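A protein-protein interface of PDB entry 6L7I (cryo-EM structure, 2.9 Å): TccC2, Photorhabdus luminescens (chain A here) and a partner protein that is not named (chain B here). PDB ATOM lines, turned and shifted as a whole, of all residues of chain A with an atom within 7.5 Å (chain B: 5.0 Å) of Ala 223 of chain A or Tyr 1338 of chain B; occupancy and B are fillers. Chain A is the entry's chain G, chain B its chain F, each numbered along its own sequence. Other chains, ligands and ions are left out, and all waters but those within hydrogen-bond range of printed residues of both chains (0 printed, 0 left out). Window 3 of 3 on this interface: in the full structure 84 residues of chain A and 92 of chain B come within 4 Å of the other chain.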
ATOM      1  N   SER A 177      -4.987 -21.206  27.913  1.00  0.00           N
ATOM      2  CA  SER A 177      -4.190 -22.089  27.083  1.00  0.00           C
ATOM      3  C   SER A 177      -2.709 -21.826  27.317  1.00  0.00           C
ATOM      4  O   SER A 177      -2.319 -20.918  28.053  1.00  0.00           O
ATOM      5  CB  SER A 177      -4.547 -21.905  25.614  1.00  0.00           C
ATOM      6  OG  SER A 177      -4.199 -20.614  25.165  1.00  0.00           O
ATOM      7  N   LEU A 178      -1.863 -22.623  26.666  1.00  0.00           N
ATOM      8  CA  LEU A 178      -0.425 -22.462  26.823  1.00  0.00           C
ATOM      9  C   LEU A 178       0.098 -21.207  26.137  1.00  0.00           C
ATOM     10  O   LEU A 178       1.233 -20.799  26.401  1.00  0.00           O
ATOM     11  CB  LEU A 178       0.300 -23.692  26.288  1.00  0.00           C
ATOM     12  CG  LEU A 178      -0.042 -25.018  26.961  1.00  0.00           C
ATOM     13  CD1 LEU A 178       0.455 -26.169  26.121  1.00  0.00           C
ATOM     14  CD2 LEU A 178       0.563 -25.075  28.333  1.00  0.00           C
ATOM     15  N   ALA A 179      -0.696 -20.592  25.260  1.00  0.00           N
ATOM     16  CA  ALA A 179      -0.336 -19.295  24.708  1.00  0.00           C
ATOM     17  C   ALA A 179      -0.777 -18.166  25.625  1.00  0.00           C
ATOM     18  O   ALA A 179      -0.068 -17.164  25.766  1.00  0.00           O
ATOM     19  CB  ALA A 179      -0.946 -19.124  23.319  1.00  0.00           C
ATOM     20  N   ALA A 221      -8.334 -23.435  21.143  1.00  0.00           N
ATOM     21  CA  ALA A 221      -7.380 -22.707  20.327  1.00  0.00           C
ATOM     22  C   ALA A 221      -6.246 -23.629  19.921  1.00  0.00           C
ATOM     23  O   ALA A 221      -5.958 -24.618  20.597  1.00  0.00           O
ATOM     24  CB  ALA A 221      -6.826 -21.492  21.068  1.00  0.00           C
ATOM     25  N   ASP A 222      -5.595 -23.294  18.813  1.00  0.00           N
ATOM     26  CA  ASP A 222      -4.469 -24.080  18.334  1.00  0.00           C
ATOM     27  C   ASP A 222      -3.197 -23.636  19.057  1.00  0.00           C
ATOM     28  O   ASP A 222      -3.238 -22.880  20.030  1.00  0.00           O
ATOM     29  CB  ASP A 222      -4.358 -23.974  16.816  1.00  0.00           C
ATOM     30  CG  ASP A 222      -4.545 -22.563  16.309  1.00  0.00           C
ATOM     31  OD1 ASP A 222      -4.454 -21.617  17.108  1.00  0.00           O
ATOM     32  OD2 ASP A 222      -4.786 -22.394  15.097  1.00  0.00           O
ATOM     33  N   ALA A 223      -2.043 -24.103  18.584  1.00  0.00           N
ATOM     34  CA  ALA A 223      -0.786 -23.728  19.217  1.00  0.00           C
ATOM     35  C   ALA A 223      -0.395 -22.289  18.924  1.00  0.00           C
ATOM     36  O   ALA A 223       0.404 -21.713  19.665  1.00  0.00           O
ATOM     37  CB  ALA A 223       0.327 -24.662  18.764  1.00  0.00           C
ATOM     38  N   THR A 224      -0.928 -21.701  17.864  1.00  0.00           N
ATOM     39  CA  THR A 224      -0.669 -20.311  17.539  1.00  0.00           C
ATOM     40  C   THR A 224      -1.602 -19.356  18.266  1.00  0.00           C
ATOM     41  O   THR A 224      -1.513 -18.144  18.057  1.00  0.00           O
ATOM     42  CB  THR A 224      -0.778 -20.100  16.032  1.00  0.00           C
ATOM     43  OG1 THR A 224      -2.077 -20.506  15.590  1.00  0.00           O
ATOM     44  CG2 THR A 224       0.266 -20.917  15.316  1.00  0.00           C
ATOM     45  N   GLY A 225      -2.492 -19.870  19.108  1.00  0.00           N
ATOM     46  CA  GLY A 225      -3.373 -19.027  19.878  1.00  0.00           C
ATOM     47  C   GLY A 225      -4.563 -18.483  19.130  1.00  0.00           C
ATOM     48  O   GLY A 225      -5.339 -17.718  19.708  1.00  0.00           O
ATOM     49  N   ALA A 226      -4.730 -18.833  17.861  1.00  0.00           N
ATOM     50  CA  ALA A 226      -5.920 -18.428  17.136  1.00  0.00           C
ATOM     51  C   ALA A 226      -7.093 -19.271  17.599  1.00  0.00           C
ATOM     52  O   ALA A 226      -6.948 -20.462  17.876  1.00  0.00           O
ATOM     53  CB  ALA A 226      -5.715 -18.578  15.632  1.00  0.00           C
ATOM     54  N   LEU A 228     -10.007 -21.563  17.502  1.00  0.00           N
ATOM     55  CA  LEU A 228     -10.546 -22.552  16.577  1.00  0.00           C
ATOM     56  C   LEU A 228     -12.061 -22.606  16.664  1.00  0.00           C
ATOM     57  O   LEU A 228     -12.761 -22.365  15.677  1.00  0.00           O
ATOM     58  CB  LEU A 228      -9.955 -23.929  16.869  1.00  0.00           C
ATOM     59  CG  LEU A 228      -8.614 -24.266  16.234  1.00  0.00           C
ATOM     60  CD1 LEU A 228      -7.976 -25.408  16.981  1.00  0.00           C
ATOM     61  CD2 LEU A 228      -8.803 -24.620  14.783  1.00  0.00           C
ATOM     62  N   PHE B1218       6.937 -26.562  22.856  1.00  0.00           N
ATOM     63  CA  PHE B1218       6.467 -26.242  24.192  1.00  0.00           C
ATOM     64  C   PHE B1218       5.395 -27.241  24.593  1.00  0.00           C
ATOM     65  O   PHE B1218       4.669 -27.768  23.748  1.00  0.00           O
ATOM     66  CB  PHE B1218       5.949 -24.798  24.319  1.00  0.00           C
ATOM     67  CG  PHE B1218       4.798 -24.461  23.420  1.00  0.00           C
ATOM     68  CD1 PHE B1218       5.017 -24.017  22.133  1.00  0.00           C
ATOM     69  CD2 PHE B1218       3.497 -24.530  23.885  1.00  0.00           C
ATOM     70  CE1 PHE B1218       3.965 -23.686  21.316  1.00  0.00           C
ATOM     71  CE2 PHE B1218       2.441 -24.204  23.070  1.00  0.00           C
ATOM     72  CZ  PHE B1218       2.678 -23.779  21.787  1.00  0.00           C
ATOM     73  N   GLU B1222      -2.708 -27.784  30.646  1.00  0.00           N
ATOM     74  CA  GLU B1222      -3.581 -26.732  30.137  1.00  0.00           C
ATOM     75  C   GLU B1222      -4.989 -26.782  30.703  1.00  0.00           C
ATOM     76  O   GLU B1222      -5.528 -25.742  31.100  1.00  0.00           O
ATOM     77  CB  GLU B1222      -3.629 -26.808  28.613  1.00  0.00           C
ATOM     78  CG  GLU B1222      -4.521 -25.811  27.928  1.00  0.00           C
ATOM     79  CD  GLU B1222      -4.645 -26.107  26.456  1.00  0.00           C
ATOM     80  OE1 GLU B1222      -4.512 -27.287  26.084  1.00  0.00           O
ATOM     81  OE2 GLU B1222      -4.866 -25.172  25.669  1.00  0.00           O
ATOM     82  N   THR B1227      -0.557 -31.659  27.759  1.00  0.00           N
ATOM     83  CA  THR B1227      -0.710 -31.395  26.338  1.00  0.00           C
ATOM     84  C   THR B1227       0.511 -30.653  25.823  1.00  0.00           C
ATOM     85  O   THR B1227       1.449 -30.362  26.567  1.00  0.00           O
ATOM     86  CB  THR B1227      -1.962 -30.570  26.060  1.00  0.00           C
ATOM     87  OG1 THR B1227      -2.139 -30.449  24.646  1.00  0.00           O
ATOM     88  CG2 THR B1227      -1.796 -29.202  26.643  1.00  0.00           C
ATOM     89  N   GLY B1228       0.484 -30.337  24.532  1.00  0.00           N
ATOM     90  CA  GLY B1228       1.538 -29.569  23.911  1.00  0.00           C
ATOM     91  C   GLY B1228       2.245 -30.360  22.838  1.00  0.00           C
ATOM     92  O   GLY B1228       1.728 -31.368  22.352  1.00  0.00           O
ATOM     93  N   TYR B1229       3.426 -29.905  22.456  1.00  0.00           N
ATOM     94  CA  TYR B1229       4.256 -30.667  21.547  1.00  0.00           C
ATOM     95  C   TYR B1229       5.020 -31.725  22.323  1.00  0.00           C
ATOM     96  O   TYR B1229       5.407 -31.518  23.473  1.00  0.00           O
ATOM     97  CB  TYR B1229       5.231 -29.752  20.817  1.00  0.00           C
ATOM     98  CG  TYR B1229       4.579 -28.796  19.858  1.00  0.00           C
ATOM     99  CD1 TYR B1229       4.332 -29.166  18.550  1.00  0.00           C
ATOM    100  CD2 TYR B1229       4.220 -27.524  20.260  1.00  0.00           C
ATOM    101  CE1 TYR B1229       3.742 -28.296  17.668  1.00  0.00           C
ATOM    102  CE2 TYR B1229       3.630 -26.645  19.387  1.00  0.00           C
ATOM    103  CZ  TYR B1229       3.394 -27.036  18.092  1.00  0.00           C
ATOM    104  OH  TYR B1229       2.806 -26.161  17.214  1.00  0.00           O
ATOM    105  N   THR B1335       3.962 -24.198  12.617  1.00  0.00           N
ATOM    106  CA  THR B1335       2.839 -25.116  12.548  1.00  0.00           C
ATOM    107  C   THR B1335       1.630 -24.541  13.274  1.00  0.00           C
ATOM    108  O   THR B1335       1.761 -23.723  14.186  1.00  0.00           O
ATOM    109  CB  THR B1335       3.204 -26.469  13.150  1.00  0.00           C
ATOM    110  OG1 THR B1335       3.214 -26.367  14.575  1.00  0.00           O
ATOM    111  CG2 THR B1335       4.570 -26.893  12.678  1.00  0.00           C
ATOM    112  N   ASP B1336       0.444 -24.981  12.857  1.00  0.00           N
ATOM    113  CA  ASP B1336      -0.790 -24.477  13.444  1.00  0.00           C
ATOM    114  C   ASP B1336      -1.084 -25.155  14.772  1.00  0.00           C
ATOM    115  O   ASP B1336      -1.187 -24.494  15.808  1.00  0.00           O
ATOM    116  CB  ASP B1336      -1.956 -24.681  12.475  1.00  0.00           C
ATOM    117  CG  ASP B1336      -2.008 -23.625  11.387  1.00  0.00           C
ATOM    118  OD1 ASP B1336      -1.058 -22.825  11.278  1.00  0.00           O
ATOM    119  OD2 ASP B1336      -3.004 -23.593  10.636  1.00  0.00           O
ATOM    120  N   ARG B1337      -1.230 -26.473  14.762  1.00  0.00           N
ATOM    121  CA  ARG B1337      -1.630 -27.236  15.935  1.00  0.00           C
ATOM    122  C   ARG B1337      -0.492 -28.143  16.388  1.00  0.00           C
ATOM    123  O   ARG B1337       0.560 -28.221  15.755  1.00  0.00           O
ATOM    124  CB  ARG B1337      -2.889 -28.047  15.642  1.00  0.00           C
ATOM    125  CG  ARG B1337      -3.840 -27.348  14.705  1.00  0.00           C
ATOM    126  CD  ARG B1337      -5.236 -27.874  14.861  1.00  0.00           C
ATOM    127  NE  ARG B1337      -6.074 -27.542  13.722  1.00  0.00           N
ATOM    128  CZ  ARG B1337      -7.385 -27.726  13.699  1.00  0.00           C
ATOM    129  NH1 ARG B1337      -7.994 -28.230  14.757  1.00  0.00           N
ATOM    130  NH2 ARG B1337      -8.086 -27.405  12.623  1.00  0.00           N
ATOM    131  N   TYR B1338      -0.715 -28.829  17.503  1.00  0.00           N
ATOM    132  CA  TYR B1338       0.302 -29.700  18.066  1.00  0.00           C
ATOM    133  C   TYR B1338       0.454 -30.967  17.231  1.00  0.00           C
ATOM    134  O   TYR B1338      -0.399 -31.315  16.412  1.00  0.00           O
ATOM    135  CB  TYR B1338      -0.044 -30.087  19.501  1.00  0.00           C
ATOM    136  CG  TYR B1338      -0.456 -28.948  20.396  1.00  0.00           C
ATOM    137  CD1 TYR B1338       0.441 -27.948  20.739  1.00  0.00           C
ATOM    138  CD2 TYR B1338      -1.734 -28.891  20.924  1.00  0.00           C
ATOM    139  CE1 TYR B1338       0.069 -26.910  21.569  1.00  0.00           C
ATOM    140  CE2 TYR B1338      -2.116 -27.857  21.757  1.00  0.00           C
ATOM    141  CZ  TYR B1338      -1.211 -26.870  22.074  1.00  0.00           C
ATOM    142  OH  TYR B1338      -1.594 -25.839  22.902  1.00  0.00           O
ATOM    143  N   ASP B1339       1.568 -31.660  17.447  1.00  0.00           N
ATOM    144  CA  ASP B1339       1.726 -32.982  16.873  1.00  0.00           C
ATOM    145  C   ASP B1339       0.799 -33.955  17.586  1.00  0.00           C
ATOM    146  O   ASP B1339       0.315 -33.682  18.685  1.00  0.00           O
ATOM    147  CB  ASP B1339       3.173 -33.455  16.978  1.00  0.00           C
ATOM    148  CG  ASP B1339       3.640 -33.595  18.409  1.00  0.00           C
ATOM    149  OD1 ASP B1339       4.526 -34.433  18.665  1.00  0.00           O
ATOM    150  OD2 ASP B1339       3.137 -32.861  19.281  1.00  0.00           O
ATOM    151  N   ARG B1340       0.537 -35.082  16.917  1.00  0.00           N
ATOM    152  CA  ARG B1340      -0.441 -36.158  17.171  1.00  0.00           C
ATOM    153  C   ARG B1340      -1.864 -35.687  16.862  1.00  0.00           C
ATOM    154  O   ARG B1340      -2.790 -36.510  16.860  1.00  0.00           O
ATOM    155  CB  ARG B1340      -0.342 -36.778  18.583  1.00  0.00           C
ATOM    156  CG  ARG B1340      -1.272 -36.253  19.683  1.00  0.00           C
ATOM    157  CD  ARG B1340      -0.728 -36.624  21.058  1.00  0.00           C
ATOM    158  NE  ARG B1340      -1.536 -36.082  22.149  1.00  0.00           N
ATOM    159  CZ  ARG B1340      -1.147 -35.107  22.965  1.00  0.00           C
ATOM    160  NH1 ARG B1340       0.050 -34.551  22.827  1.00  0.00           N
ATOM    161  NH2 ARG B1340      -1.955 -34.688  23.928  1.00  0.00           N
ATOM    162  N   ASP B1341      -2.060 -34.414  16.538  1.00  0.00           N
ATOM    163  CA  ASP B1341      -3.289 -33.904  15.955  1.00  0.00           C
ATOM    164  C   ASP B1341      -3.100 -33.949  14.445  1.00  0.00           C
ATOM    165  O   ASP B1341      -2.183 -33.317  13.912  1.00  0.00           O
ATOM    166  CB  ASP B1341      -3.565 -32.484  16.442  1.00  0.00           C
ATOM    167  CG  ASP B1341      -4.904 -31.939  15.981  1.00  0.00           C
ATOM    168  OD1 ASP B1341      -5.200 -30.783  16.338  1.00  0.00           O
ATOM    169  OD2 ASP B1341      -5.682 -32.652  15.314  1.00  0.00           O
ATOM    170  N   GLN B1344      -2.765 -30.795  11.549  1.00  0.00           N
ATOM    171  CA  GLN B1344      -1.715 -29.790  11.590  1.00  0.00           C
ATOM    172  C   GLN B1344      -1.197 -29.505  10.190  1.00  0.00           C
ATOM    173  O   GLN B1344      -0.779 -30.419   9.475  1.00  0.00           O
ATOM    174  CB  GLN B1344      -0.572 -30.252  12.489  1.00  0.00           C
ATOM    175  CG  GLN B1344       0.712 -29.482  12.292  1.00  0.00           C
ATOM    176  CD  GLN B1344       1.871 -30.085  13.029  1.00  0.00           C
ATOM    177  OE1 GLN B1344       2.915 -30.350  12.453  1.00  0.00           O
ATOM    178  NE2 GLN B1344       1.697 -30.299  14.316  1.00  0.00           N
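The side-chain hydroxyl (OG1) of Thr 1335 of chain B lies within hydrogen-bond range of the side-chain hydroxyl (OH) of Tyr 1229 of chain B (2.7 Å). The backbone carbonyl oxygen (O) of Arg 1337 of chain B is in hydrogen-bond range of the side-chain hydroxyl (OH) of Tyr 1229 of chain B. OG1 of Thr 1335 of chain B is in hydrogen-bond range of O of Arg 1337 of chain B (3.4 Å). The backbone carbonyl oxygen (O) of Tyr 1338 of chain B is in hydrogen-bond range of the side-chain amide nitrogen (NE2) of Gln 1344 of chain B (3.1 Å). OG1 of Thr 224 of chain A lies within hydrogen-bond range of OD1 of Asp 222 of chain A, 3.0 Å away. OD1 of Asp 222 of chain A lies within hydrogen-bond range of N of Gly 225 of chain A, at 3.3 Å.
Of the 13 printed residues of chain B, 8 touch a printed residue of chain A. Hydrophobic or aromatic side chains of chain B that line the printed part of chain A: Phe 1218, Tyr 1229 and Tyr 1338. Hydrophobic or aromatic side chains of chain A within 4 Å of the printed part of chain B: Leu 178, Ala 223 and Leu 228. Among the printed residues, 12 pairs touch across the chains. Among the printed residues, no Asp or Glu carboxylate lies within 4 Å of a Lys or Arg side-chain nitrogen of the other chain.
O of Asp 1336 of chain B is in hydrogen-bond range of N of Ala 223 of chain A (2.9 Å). O of Asp 1336 of chain B sits at hydrogen-bond distance from N of Thr 224 of chain A (3.5 Å).
Of chain B, only Phe 1218, Tyr 1229, Asp 1336 and Tyr 1338 come within 4 Å of Ala 223 of chain A. Tyr 1338 of chain B touches just these residues of chain A: Leu 178 and Ala 223. Of the printed residues of chain A, Thr 1335 of chain B touches Thr 224. Of the printed residues of chain A, Phe 1218 of chain B touches Leu 178 and Ala 223. Printed residues of chain A within 4 Å of Asp 1336 of chain B: Asp 222, Ala 223 and Thr 224. Arg 1340 of chain B touches none of the printed residues of chain A. The nearest residue of chain A that does not touch Tyr 1338 of chain B is Asp 222 of chain A (4.4 Å). The nearest printed residue of chain A that does not touch Thr 1335 of chain B is Ala 223 of chain A (4.9 Å).
Ser 177 of chain A touches Glu 1222 of chain B. CE2 of Phe 1218 of chain B touches CB of Leu 178 of chain A, 3.9 Å away. Leu 178 of chain A touches Thr 1227 of chain B. Leu 178 of chain A touches Tyr 1338 of chain B (CD1 to OH, 3.8 Å). O of Asp 1336 of chain B touches CB of Asp 222 of chain A (3.4 Å). CZ of Phe 1218 of chain B touches O of Ala 223 of chain A, 3.7 Å away. Ala 223 of chain A touches Tyr 1229 of chain B. CE1 of Tyr 1338 of chain B touches CB of Ala 223 of chain A (3.6 Å). Thr 224 of chain A touches Thr 1335 of chain B. CZ of Arg 1337 of chain B touches CD2 of Leu 228 of chain A (3.6 Å).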
